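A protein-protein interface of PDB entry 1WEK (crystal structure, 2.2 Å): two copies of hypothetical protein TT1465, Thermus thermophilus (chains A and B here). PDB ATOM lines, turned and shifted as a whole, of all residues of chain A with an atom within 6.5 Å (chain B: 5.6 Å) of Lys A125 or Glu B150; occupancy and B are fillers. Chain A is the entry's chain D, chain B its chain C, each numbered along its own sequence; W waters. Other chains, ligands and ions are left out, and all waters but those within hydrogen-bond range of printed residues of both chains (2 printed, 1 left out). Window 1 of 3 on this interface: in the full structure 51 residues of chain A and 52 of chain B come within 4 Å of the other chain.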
ATOM      1  N   LEU A  98     -18.174  -2.076  14.443  1.00  0.00           N
ATOM      2  CA  LEU A  98     -18.476  -3.453  14.075  1.00  0.00           C
ATOM      3  C   LEU A  98     -19.337  -3.938  15.231  1.00  0.00           C
ATOM      4  O   LEU A  98     -18.871  -4.643  16.128  1.00  0.00           O
ATOM      5  CB  LEU A  98     -17.193  -4.273  13.951  1.00  0.00           C
ATOM      6  CG  LEU A  98     -16.216  -3.779  12.882  1.00  0.00           C
ATOM      7  CD1 LEU A  98     -15.104  -4.806  12.713  1.00  0.00           C
ATOM      8  CD2 LEU A  98     -16.942  -3.542  11.562  1.00  0.00           C
ATOM      9  N   LEU A 118     -23.501  -6.912  13.014  1.00  0.00           N
ATOM     10  CA  LEU A 118     -22.920  -8.257  13.031  1.00  0.00           C
ATOM     11  C   LEU A 118     -23.478  -9.169  14.109  1.00  0.00           C
ATOM     12  O   LEU A 118     -23.761  -8.737  15.225  1.00  0.00           O
ATOM     13  CB  LEU A 118     -21.414  -8.153  13.235  1.00  0.00           C
ATOM     14  CG  LEU A 118     -20.651  -7.321  12.208  1.00  0.00           C
ATOM     15  CD1 LEU A 118     -19.173  -7.277  12.584  1.00  0.00           C
ATOM     16  CD2 LEU A 118     -20.850  -7.929  10.825  1.00  0.00           C
ATOM     17  N   TYR A 120     -22.158 -12.605  14.199  1.00  0.00           N
ATOM     18  CA  TYR A 120     -21.133 -13.609  14.383  1.00  0.00           C
ATOM     19  C   TYR A 120     -19.745 -13.104  14.760  1.00  0.00           C
ATOM     20  O   TYR A 120     -19.074 -12.408  13.997  1.00  0.00           O
ATOM     21  CB  TYR A 120     -21.087 -14.510  13.136  1.00  0.00           C
ATOM     22  CG  TYR A 120     -22.377 -15.294  12.965  1.00  0.00           C
ATOM     23  CD1 TYR A 120     -23.428 -14.795  12.197  1.00  0.00           C
ATOM     24  CD2 TYR A 120     -22.576 -16.508  13.644  1.00  0.00           C
ATOM     25  CE1 TYR A 120     -24.645 -15.474  12.105  1.00  0.00           C
ATOM     26  CE2 TYR A 120     -23.781 -17.189  13.570  1.00  0.00           C
ATOM     27  CZ  TYR A 120     -24.812 -16.664  12.800  1.00  0.00           C
ATOM     28  OH  TYR A 120     -26.017 -17.311  12.752  1.00  0.00           O
ATOM     29  N   PHE A 121     -19.325 -13.488  15.959  1.00  0.00           N
ATOM     30  CA  PHE A 121     -18.039 -13.103  16.496  1.00  0.00           C
ATOM     31  C   PHE A 121     -16.878 -13.368  15.536  1.00  0.00           C
ATOM     32  O   PHE A 121     -15.955 -12.559  15.461  1.00  0.00           O
ATOM     33  CB  PHE A 121     -17.802 -13.826  17.835  1.00  0.00           C
ATOM     34  CG  PHE A 121     -17.450 -15.277  17.689  1.00  0.00           C
ATOM     35  CD1 PHE A 121     -16.118 -15.680  17.634  1.00  0.00           C
ATOM     36  CD2 PHE A 121     -18.443 -16.239  17.561  1.00  0.00           C
ATOM     37  CE1 PHE A 121     -15.784 -17.018  17.448  1.00  0.00           C
ATOM     38  CE2 PHE A 121     -18.111 -17.580  17.372  1.00  0.00           C
ATOM     39  CZ  PHE A 121     -16.771 -17.968  17.315  1.00  0.00           C
ATOM     40  N   PHE A 122     -16.917 -14.473  14.787  1.00  0.00           N
ATOM     41  CA  PHE A 122     -15.811 -14.763  13.875  1.00  0.00           C
ATOM     42  C   PHE A 122     -15.783 -13.884  12.620  1.00  0.00           C
ATOM     43  O   PHE A 122     -14.727 -13.707  11.998  1.00  0.00           O
ATOM     44  CB  PHE A 122     -15.783 -16.251  13.516  1.00  0.00           C
ATOM     45  CG  PHE A 122     -16.989 -16.732  12.793  1.00  0.00           C
ATOM     46  CD1 PHE A 122     -17.058 -16.653  11.407  1.00  0.00           C
ATOM     47  CD2 PHE A 122     -18.071 -17.260  13.495  1.00  0.00           C
ATOM     48  CE1 PHE A 122     -18.188 -17.090  10.733  1.00  0.00           C
ATOM     49  CE2 PHE A 122     -19.199 -17.697  12.832  1.00  0.00           C
ATOM     50  CZ  PHE A 122     -19.262 -17.615  11.446  1.00  0.00           C
ATOM     51  N   VAL A 123     -16.929 -13.314  12.250  1.00  0.00           N
ATOM     52  CA  VAL A 123     -16.955 -12.432  11.096  1.00  0.00           C
ATOM     53  C   VAL A 123     -16.411 -11.086  11.563  1.00  0.00           C
ATOM     54  O   VAL A 123     -15.742 -10.355  10.815  1.00  0.00           O
ATOM     55  CB  VAL A 123     -18.377 -12.213  10.572  1.00  0.00           C
ATOM     56  CG1 VAL A 123     -18.336 -11.254   9.411  1.00  0.00           C
ATOM     57  CG2 VAL A 123     -18.997 -13.545  10.144  1.00  0.00           C
ATOM     58  N   ARG A 124     -16.700 -10.760  12.814  1.00  0.00           N
ATOM     59  CA  ARG A 124     -16.248  -9.498  13.370  1.00  0.00           C
ATOM     60  C   ARG A 124     -14.737  -9.512  13.517  1.00  0.00           C
ATOM     61  O   ARG A 124     -14.082  -8.502  13.272  1.00  0.00           O
ATOM     62  CB  ARG A 124     -16.882  -9.270  14.734  1.00  0.00           C
ATOM     63  CG  ARG A 124     -16.669  -7.888  15.302  1.00  0.00           C
ATOM     64  CD  ARG A 124     -16.765  -7.995  16.795  1.00  0.00           C
ATOM     65  NE  ARG A 124     -17.494  -6.889  17.395  1.00  0.00           N
ATOM     66  CZ  ARG A 124     -17.574  -6.682  18.704  1.00  0.00           C
ATOM     67  NH1 ARG A 124     -16.967  -7.504  19.545  1.00  0.00           N
ATOM     68  NH2 ARG A 124     -18.260  -5.649  19.166  1.00  0.00           N
ATOM     69  N   LYS A 125     -14.195 -10.662  13.915  1.00  0.00           N
ATOM     70  CA  LYS A 125     -12.753 -10.809  14.106  1.00  0.00           C
ATOM     71  C   LYS A 125     -12.009 -10.615  12.788  1.00  0.00           C
ATOM     72  O   LYS A 125     -10.957  -9.979  12.750  1.00  0.00           O
ATOM     73  CB  LYS A 125     -12.416 -12.196  14.674  1.00  0.00           C
ATOM     74  CG  LYS A 125     -13.005 -12.524  16.045  1.00  0.00           C
ATOM     75  CD  LYS A 125     -12.161 -11.971  17.170  1.00  0.00           C
ATOM     76  CE  LYS A 125     -12.627 -12.477  18.535  1.00  0.00           C
ATOM     77  NZ  LYS A 125     -12.398 -13.936  18.721  1.00  0.00           N
ATOM     78  N   VAL A 126     -12.535 -11.186  11.709  1.00  0.00           N
ATOM     79  CA  VAL A 126     -11.889 -11.031  10.409  1.00  0.00           C
ATOM     80  C   VAL A 126     -11.927  -9.547  10.005  1.00  0.00           C
ATOM     81  O   VAL A 126     -10.905  -8.969   9.645  1.00  0.00           O
ATOM     82  CB  VAL A 126     -12.592 -11.912   9.314  1.00  0.00           C
ATOM     83  CG1 VAL A 126     -12.080 -11.555   7.924  1.00  0.00           C
ATOM     84  CG2 VAL A 126     -12.348 -13.390   9.600  1.00  0.00           C
ATOM     85  N   LEU A 127     -13.098  -8.925  10.096  1.00  0.00           N
ATOM     86  CA  LEU A 127     -13.232  -7.519   9.710  1.00  0.00           C
ATOM     87  C   LEU A 127     -12.378  -6.569  10.540  1.00  0.00           C
ATOM     88  O   LEU A 127     -12.036  -5.483  10.084  1.00  0.00           O
ATOM     89  CB  LEU A 127     -14.704  -7.092   9.775  1.00  0.00           C
ATOM     90  CG  LEU A 127     -15.631  -7.873   8.830  1.00  0.00           C
ATOM     91  CD1 LEU A 127     -17.055  -7.417   9.032  1.00  0.00           C
ATOM     92  CD2 LEU A 127     -15.200  -7.651   7.367  1.00  0.00           C
ATOM     93  N   PHE A 128     -12.021  -6.979  11.753  1.00  0.00           N
ATOM     94  CA  PHE A 128     -11.193  -6.149  12.631  1.00  0.00           C
ATOM     95  C   PHE A 128      -9.765  -5.997  12.095  1.00  0.00           C
ATOM     96  O   PHE A 128      -9.155  -4.943  12.238  1.00  0.00           O
ATOM     97  CB  PHE A 128     -11.126  -6.761  14.041  1.00  0.00           C
ATOM     98  CG  PHE A 128     -12.011  -6.087  15.051  1.00  0.00           C
ATOM     99  CD1 PHE A 128     -12.820  -6.843  15.895  1.00  0.00           C
ATOM    100  CD2 PHE A 128     -12.005  -4.701  15.194  1.00  0.00           C
ATOM    101  CE1 PHE A 128     -13.610  -6.223  16.870  1.00  0.00           C
ATOM    102  CE2 PHE A 128     -12.787  -4.076  16.164  1.00  0.00           C
ATOM    103  CZ  PHE A 128     -13.588  -4.830  17.002  1.00  0.00           C
ATOM    104  N   VAL A 129      -9.239  -7.042  11.468  1.00  0.00           N
ATOM    105  CA  VAL A 129      -7.861  -6.999  10.962  1.00  0.00           C
ATOM    106  C   VAL A 129      -7.635  -6.969   9.441  1.00  0.00           C
ATOM    107  O   VAL A 129      -6.544  -6.636   8.979  1.00  0.00           O
ATOM    108  CB  VAL A 129      -7.065  -8.181  11.532  1.00  0.00           C
ATOM    109  CG1 VAL A 129      -7.197  -8.187  13.036  1.00  0.00           C
ATOM    110  CG2 VAL A 129      -7.581  -9.505  10.954  1.00  0.00           C
ATOM    111  N   ARG A 130      -8.667  -7.300   8.675  1.00  0.00           N
ATOM    112  CA  ARG A 130      -8.579  -7.344   7.221  1.00  0.00           C
ATOM    113  C   ARG A 130      -7.965  -6.118   6.565  1.00  0.00           C
ATOM    114  O   ARG A 130      -7.262  -6.238   5.559  1.00  0.00           O
ATOM    115  CB  ARG A 130      -9.969  -7.578   6.616  1.00  0.00           C
ATOM    116  CG  ARG A 130      -9.993  -7.593   5.095  1.00  0.00           C
ATOM    117  CD  ARG A 130      -9.009  -8.625   4.560  1.00  0.00           C
ATOM    118  NE  ARG A 130      -8.960  -8.660   3.103  1.00  0.00           N
ATOM    119  CZ  ARG A 130      -8.301  -7.788   2.343  1.00  0.00           C
ATOM    120  NH1 ARG A 130      -7.615  -6.788   2.892  1.00  0.00           N
ATOM    121  NH2 ARG A 130      -8.317  -7.930   1.022  1.00  0.00           N
ATOM    122  N   PHE A 135      -3.478  -1.602  15.466  1.00  0.00           N
ATOM    123  CA  PHE A 135      -4.505  -2.003  16.410  1.00  0.00           C
ATOM    124  C   PHE A 135      -4.105  -1.485  17.795  1.00  0.00           C
ATOM    125  O   PHE A 135      -2.985  -1.721  18.265  1.00  0.00           O
ATOM    126  CB  PHE A 135      -4.639  -3.530  16.411  1.00  0.00           C
ATOM    127  CG  PHE A 135      -6.050  -4.014  16.599  1.00  0.00           C
ATOM    128  CD1 PHE A 135      -6.550  -5.057  15.816  1.00  0.00           C
ATOM    129  CD2 PHE A 135      -6.886  -3.431  17.557  1.00  0.00           C
ATOM    130  CE1 PHE A 135      -7.859  -5.514  15.985  1.00  0.00           C
ATOM    131  CE2 PHE A 135      -8.193  -3.878  17.733  1.00  0.00           C
ATOM    132  CZ  PHE A 135      -8.684  -4.921  16.946  1.00  0.00           C
ATOM    133  N   GLY A 143     -13.753  -9.390  26.715  1.00  0.00           N
ATOM    134  CA  GLY A 143     -13.774  -8.996  25.318  1.00  0.00           C
ATOM    135  C   GLY A 143     -12.449  -8.465  24.785  1.00  0.00           C
ATOM    136  O   GLY A 143     -11.970  -8.897  23.731  1.00  0.00           O
ATOM    137  N   ASP A 146      -9.760 -11.142  24.645  1.00  0.00           N
ATOM    138  CA  ASP A 146     -10.102 -12.051  23.558  1.00  0.00           C
ATOM    139  C   ASP A 146      -9.604 -11.500  22.232  1.00  0.00           C
ATOM    140  O   ASP A 146      -8.877 -12.173  21.509  1.00  0.00           O
ATOM    141  CB  ASP A 146     -11.623 -12.261  23.538  1.00  0.00           C
ATOM    142  CG  ASP A 146     -12.114 -13.034  22.315  1.00  0.00           C
ATOM    143  OD1 ASP A 146     -11.495 -14.047  21.917  1.00  0.00           O
ATOM    144  OD2 ASP A 146     -13.155 -12.626  21.762  1.00  0.00           O
ATOM    145  N   GLU A 147      -9.976 -10.263  21.937  1.00  0.00           N
ATOM    146  CA  GLU A 147      -9.563  -9.620  20.701  1.00  0.00           C
ATOM    147  C   GLU A 147      -8.047  -9.435  20.611  1.00  0.00           C
ATOM    148  O   GLU A 147      -7.480  -9.477  19.516  1.00  0.00           O
ATOM    149  CB  GLU A 147     -10.262  -8.266  20.558  1.00  0.00           C
ATOM    150  CG  GLU A 147      -9.958  -7.555  19.250  1.00  0.00           C
ATOM    151  CD  GLU A 147     -10.154  -8.450  18.030  1.00  0.00           C
ATOM    152  OE1 GLU A 147      -9.379  -8.297  17.059  1.00  0.00           O
ATOM    153  OE2 GLU A 147     -11.079  -9.298  18.042  1.00  0.00           O
ATOM    154  N   SER A 149      -5.700 -11.431  22.143  1.00  0.00           N
ATOM    155  CA  SER A 149      -5.179 -12.783  21.919  1.00  0.00           C
ATOM    156  C   SER A 149      -5.307 -13.155  20.441  1.00  0.00           C
ATOM    157  O   SER A 149      -4.385 -13.713  19.845  1.00  0.00           O
ATOM    158  CB  SER A 149      -5.982 -13.803  22.728  1.00  0.00           C
ATOM    159  OG  SER A 149      -5.941 -13.503  24.099  1.00  0.00           O
ATOM    160  N   GLU A 150      -6.468 -12.858  19.865  1.00  0.00           N
ATOM    161  CA  GLU A 150      -6.720 -13.155  18.460  1.00  0.00           C
ATOM    162  C   GLU A 150      -5.666 -12.499  17.585  1.00  0.00           C
ATOM    163  O   GLU A 150      -4.983 -13.161  16.801  1.00  0.00           O
ATOM    164  CB  GLU A 150      -8.098 -12.640  18.045  1.00  0.00           C
ATOM    165  CG  GLU A 150      -9.192 -13.681  18.018  1.00  0.00           C
ATOM    166  CD  GLU A 150      -9.100 -14.598  16.811  1.00  0.00           C
ATOM    167  OE1 GLU A 150      -8.900 -14.084  15.688  1.00  0.00           O
ATOM    168  OE2 GLU A 150      -9.244 -15.829  16.980  1.00  0.00           O
ATOM    169  N   LEU A 154      -2.903 -14.284  15.057  1.00  0.00           N
ATOM    170  CA  LEU A 154      -2.979 -14.098  13.610  1.00  0.00           C
ATOM    171  C   LEU A 154      -1.646 -13.527  13.108  1.00  0.00           C
ATOM    172  O   LEU A 154      -1.149 -13.926  12.052  1.00  0.00           O
ATOM    173  CB  LEU A 154      -4.132 -13.138  13.248  1.00  0.00           C
ATOM    174  CG  LEU A 154      -5.580 -13.442  13.697  1.00  0.00           C
ATOM    175  CD1 LEU A 154      -6.469 -12.285  13.284  1.00  0.00           C
ATOM    176  CD2 LEU A 154      -6.110 -14.733  13.069  1.00  0.00           C
ATOM    177  N   LYS B 125     -13.135 -22.640  14.932  1.00  0.00           N
ATOM    178  CA  LYS B 125     -13.481 -22.040  16.219  1.00  0.00           C
ATOM    179  C   LYS B 125     -14.943 -22.312  16.581  1.00  0.00           C
ATOM    180  O   LYS B 125     -15.287 -22.472  17.753  1.00  0.00           O
ATOM    181  CB  LYS B 125     -13.226 -20.531  16.180  1.00  0.00           C
ATOM    182  CG  LYS B 125     -11.759 -20.145  16.254  1.00  0.00           C
ATOM    183  CD  LYS B 125     -11.445 -18.930  15.371  1.00  0.00           C
ATOM    184  CE  LYS B 125     -11.943 -17.620  15.969  1.00  0.00           C
ATOM    185  NZ  LYS B 125     -11.659 -16.440  15.101  1.00  0.00           N
ATOM    186  N   VAL B 126     -15.810 -22.341  15.581  1.00  0.00           N
ATOM    187  CA  VAL B 126     -17.202 -22.635  15.863  1.00  0.00           C
ATOM    188  C   VAL B 126     -17.298 -24.131  16.180  1.00  0.00           C
ATOM    189  O   VAL B 126     -17.978 -24.539  17.114  1.00  0.00           O
ATOM    190  CB  VAL B 126     -18.095 -22.258  14.664  1.00  0.00           C
ATOM    191  CG1 VAL B 126     -19.547 -22.689  14.911  1.00  0.00           C
ATOM    192  CG2 VAL B 126     -18.010 -20.758  14.450  1.00  0.00           C
ATOM    193  N   LEU B 145      -4.194 -19.318  24.713  1.00  0.00           N
ATOM    194  CA  LEU B 145      -4.813 -18.170  25.369  1.00  0.00           C
ATOM    195  C   LEU B 145      -5.930 -17.635  24.491  1.00  0.00           C
ATOM    196  O   LEU B 145      -7.016 -17.284  24.972  1.00  0.00           O
ATOM    197  CB  LEU B 145      -3.770 -17.074  25.620  1.00  0.00           C
ATOM    198  CG  LEU B 145      -4.285 -15.729  26.153  1.00  0.00           C
ATOM    199  CD1 LEU B 145      -5.091 -15.950  27.421  1.00  0.00           C
ATOM    200  CD2 LEU B 145      -3.091 -14.799  26.414  1.00  0.00           C
ATOM    201  N   ASP B 146      -5.648 -17.582  23.198  1.00  0.00           N
ATOM    202  CA  ASP B 146      -6.608 -17.129  22.197  1.00  0.00           C
ATOM    203  C   ASP B 146      -7.872 -17.988  22.293  1.00  0.00           C
ATOM    204  O   ASP B 146      -8.984 -17.456  22.323  1.00  0.00           O
ATOM    205  CB  ASP B 146      -5.973 -17.236  20.805  1.00  0.00           C
ATOM    206  CG  ASP B 146      -6.991 -17.199  19.679  1.00  0.00           C
ATOM    207  OD1 ASP B 146      -7.761 -16.223  19.591  1.00  0.00           O
ATOM    208  OD2 ASP B 146      -7.006 -18.152  18.871  1.00  0.00           O
ATOM    209  N   GLU B 147      -7.705 -19.308  22.359  1.00  0.00           N
ATOM    210  CA  GLU B 147      -8.855 -20.199  22.459  1.00  0.00           C
ATOM    211  C   GLU B 147      -9.546 -20.023  23.809  1.00  0.00           C
ATOM    212  O   GLU B 147     -10.765 -20.070  23.885  1.00  0.00           O
ATOM    213  CB  GLU B 147      -8.444 -21.664  22.316  1.00  0.00           C
ATOM    214  CG  GLU B 147      -9.095 -22.419  21.170  1.00  0.00           C
ATOM    215  CD  GLU B 147     -10.608 -22.270  21.101  1.00  0.00           C
ATOM    216  OE1 GLU B 147     -11.320 -22.723  22.019  1.00  0.00           O
ATOM    217  OE2 GLU B 147     -11.092 -21.694  20.111  1.00  0.00           O
ATOM    218  N   LEU B 148      -8.773 -19.832  24.876  1.00  0.00           N
ATOM    219  CA  LEU B 148      -9.380 -19.655  26.195  1.00  0.00           C
ATOM    220  C   LEU B 148     -10.227 -18.376  26.208  1.00  0.00           C
ATOM    221  O   LEU B 148     -11.368 -18.389  26.646  1.00  0.00           O
ATOM    222  CB  LEU B 148      -8.307 -19.541  27.277  1.00  0.00           C
ATOM    223  CG  LEU B 148      -8.589 -20.113  28.675  1.00  0.00           C
ATOM    224  CD1 LEU B 148      -7.785 -19.314  29.664  1.00  0.00           C
ATOM    225  CD2 LEU B 148     -10.065 -20.069  29.040  1.00  0.00           C
ATOM    226  N   SER B 149      -9.650 -17.282  25.721  1.00  0.00           N
ATOM    227  CA  SER B 149     -10.319 -15.984  25.690  1.00  0.00           C
ATOM    228  C   SER B 149     -11.634 -16.067  24.954  1.00  0.00           C
ATOM    229  O   SER B 149     -12.690 -15.705  25.479  1.00  0.00           O
ATOM    230  CB  SER B 149      -9.439 -14.944  24.996  1.00  0.00           C
ATOM    231  OG  SER B 149      -8.176 -14.862  25.616  1.00  0.00           O
ATOM    232  N   GLU B 150     -11.564 -16.532  23.717  1.00  0.00           N
ATOM    233  CA  GLU B 150     -12.770 -16.657  22.919  1.00  0.00           C
ATOM    234  C   GLU B 150     -13.839 -17.428  23.697  1.00  0.00           C
ATOM    235  O   GLU B 150     -14.987 -16.991  23.794  1.00  0.00           O
ATOM    236  CB  GLU B 150     -12.461 -17.372  21.610  1.00  0.00           C
ATOM    237  CG  GLU B 150     -13.637 -17.406  20.660  1.00  0.00           C
ATOM    238  CD  GLU B 150     -13.205 -17.718  19.257  1.00  0.00           C
ATOM    239  OE1 GLU B 150     -13.323 -18.886  18.836  1.00  0.00           O
ATOM    240  OE2 GLU B 150     -12.730 -16.786  18.581  1.00  0.00           O
ATOM    241  N   VAL B 151     -13.456 -18.576  24.250  1.00  0.00           N
ATOM    242  CA  VAL B 151     -14.395 -19.381  25.016  1.00  0.00           C
ATOM    243  C   VAL B 151     -15.017 -18.561  26.163  1.00  0.00           C
ATOM    244  O   VAL B 151     -16.252 -18.486  26.295  1.00  0.00           O
ATOM    245  CB  VAL B 151     -13.701 -20.638  25.579  1.00  0.00           C
ATOM    246  CG1 VAL B 151     -14.653 -21.394  26.475  1.00  0.00           C
ATOM    247  CG2 VAL B 151     -13.252 -21.536  24.429  1.00  0.00           C
ATOM    248  N   LEU B 152     -14.165 -17.937  26.974  1.00  0.00           N
ATOM    249  CA  LEU B 152     -14.654 -17.123  28.087  1.00  0.00           C
ATOM    250  C   LEU B 152     -15.617 -16.043  27.609  1.00  0.00           C
ATOM    251  O   LEU B 152     -16.639 -15.799  28.248  1.00  0.00           O
ATOM    252  CB  LEU B 152     -13.489 -16.483  28.860  1.00  0.00           C
ATOM    253  CG  LEU B 152     -12.646 -17.413  29.742  1.00  0.00           C
ATOM    254  CD1 LEU B 152     -11.719 -16.568  30.604  1.00  0.00           C
ATOM    255  CD2 LEU B 152     -13.544 -18.268  30.648  1.00  0.00           C
ATOM    256  N   VAL B 153     -15.310 -15.403  26.483  1.00  0.00           N
ATOM    257  CA  VAL B 153     -16.198 -14.363  25.963  1.00  0.00           C
ATOM    258  C   VAL B 153     -17.529 -14.945  25.471  1.00  0.00           C
ATOM    259  O   VAL B 153     -18.585 -14.392  25.757  1.00  0.00           O
ATOM    260  CB  VAL B 153     -15.531 -13.555  24.823  1.00  0.00           C
ATOM    261  CG1 VAL B 153     -16.587 -12.782  24.038  1.00  0.00           C
ATOM    262  CG2 VAL B 153     -14.538 -12.567  25.405  1.00  0.00           C
ATOM    263  N   LEU B 154     -17.479 -16.060  24.744  1.00  0.00           N
ATOM    264  CA  LEU B 154     -18.700 -16.683  24.241  1.00  0.00           C
ATOM    265  C   LEU B 154     -19.589 -17.190  25.387  1.00  0.00           C
ATOM    266  O   LEU B 154     -20.816 -17.200  25.277  1.00  0.00           O
ATOM    267  CB  LEU B 154     -18.359 -17.844  23.305  1.00  0.00           C
ATOM    268  CG  LEU B 154     -17.618 -17.530  22.004  1.00  0.00           C
ATOM    269  CD1 LEU B 154     -17.393 -18.837  21.246  1.00  0.00           C
ATOM    270  CD2 LEU B 154     -18.430 -16.553  21.154  1.00  0.00           C
ATOM    271  N   LEU B 155     -18.960 -17.622  26.475  1.00  0.00           N
ATOM    272  CA  LEU B 155     -19.685 -18.108  27.642  1.00  0.00           C
ATOM    273  C   LEU B 155     -20.272 -16.907  28.400  1.00  0.00           C
ATOM    274  O   LEU B 155     -21.456 -16.873  28.718  1.00  0.00           O
ATOM    275  CB  LEU B 155     -18.736 -18.887  28.560  1.00  0.00           C
ATOM    276  CG  LEU B 155     -18.855 -20.412  28.693  1.00  0.00           C
ATOM    277  CD1 LEU B 155     -19.856 -20.965  27.705  1.00  0.00           C
ATOM    278  CD2 LEU B 155     -17.489 -21.041  28.492  1.00  0.00           C
HETATM  279  O   HOH W   1      -7.169 -17.155  15.762  1.00  0.00           O
HETATM  280  O   HOH W   2      -9.258 -14.930  21.331  1.00  0.00           O
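Lys A125 touches one residue of chain B. Of the printed residues of chain B, Asp A146 touches Ser B149 (3.3 Å), Glu B150 (3.1 Å) and Val B153 (3.5 Å). Of the printed residues of chain B, Phe A121 touches Glu B150 and Leu B154. Arg A130 touches none of the printed residues of chain B. Leu B155 touches none of the printed residues of chain A. The nearest residue of chain B that does not touch Lys A125 is Lys B125 (4.2 Å).
Hydrophobic or aromatic side chains of chain A that line the printed part of chain B: Phe A121 and Phe A122. Of the 13 printed residues of chain B, 8 touch a printed residue of chain A. Printed residues of chain B that touch a printed residue of chain A: Lys B125, Val B126, Leu B145, Asp B146, Ser B149, Glu B150, Val B153 and Leu B154. Hydrophobic or aromatic side chains of chain B within 4 Å of the printed part of chain A: Val B126, Leu B145, Val B153 and Leu B154. Among the printed residues, 14 pairs touch across the chains. Among the printed residues, Asp or Glu carboxylates within 4 Å of a Lys or Arg side-chain nitrogen of the other chain: Lys A125 with Glu B150 (2.9 Å) and Glu A150 with Lys B125 (3.1 Å).
Glu B150 touches Phe A121. CD2 of Leu B154 touches CD2 of Phe A121, 3.6 Å away. CD2 of Phe A122 touches CG2 of Val B126 (3.6 Å). Gly A143 touches Val B153. CA of Asp A146 touches CB of Ser B149, at 3.3 Å. Val B153 touches Asp A146 (CG2 to CB, 3.5 Å). Ser A149 touches Leu B145 (OG to CG, 3.5 Å). Ser A149 touches Asp B146 (CB to CA, 3.4 Å). Glu A150 touches Glu B150.
Water W2 bridges OD1 of Asp A146 and OD1 of Asp B146. Water W1 bridges OE2 of Glu A150 (2.7 Å) and OD2 of Asp B146 (3.3 Å).
NZ of Lys B125 is in salt-bridge range of OE2 of Glu B150 (3.7 Å). OG of Ser B149 is in hydrogen-bond range of O of Leu B145 (2.8 Å). The side-chain amino group (NZ) of Lys A125 is in salt-bridge range of the side-chain carboxylate (OD1) of Asp A146, 3.3 Å away.
Lys A125 touches Glu B150, and with the chains exchanged Glu A150 touches Lys B125. Asp A146 touches Ser B149, and with the chains exchanged Ser A149 touches Asp B146. Ser A149 touches its own counterpart, Ser B149. Glu A150 touches its own counterpart, Glu B150. Positions printed for both chains: 125, 126, 146, 147, 149, 150 and 154.
NZ of Lys B125 is in salt-bridge range of OE2 of Glu A150 (3.1 Å). The side-chain hydroxyl of Ser B149 is in hydrogen-bond range of the side-chain hydroxyl of Ser A149. NZ of Lys A125 lies within salt-bridge range of OE2 of Glu B150 (2.9 Å). The backbone NH (N) of Glu B150 sits at hydrogen-bond distance from the side-chain carboxylate (OD1) of Asp A146 (3.1 Å). The side-chain carboxylate (OD1) of Asp B146 sits close to the side-chain carboxylate (OE2) of Glu A150, 3.0 Å away.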
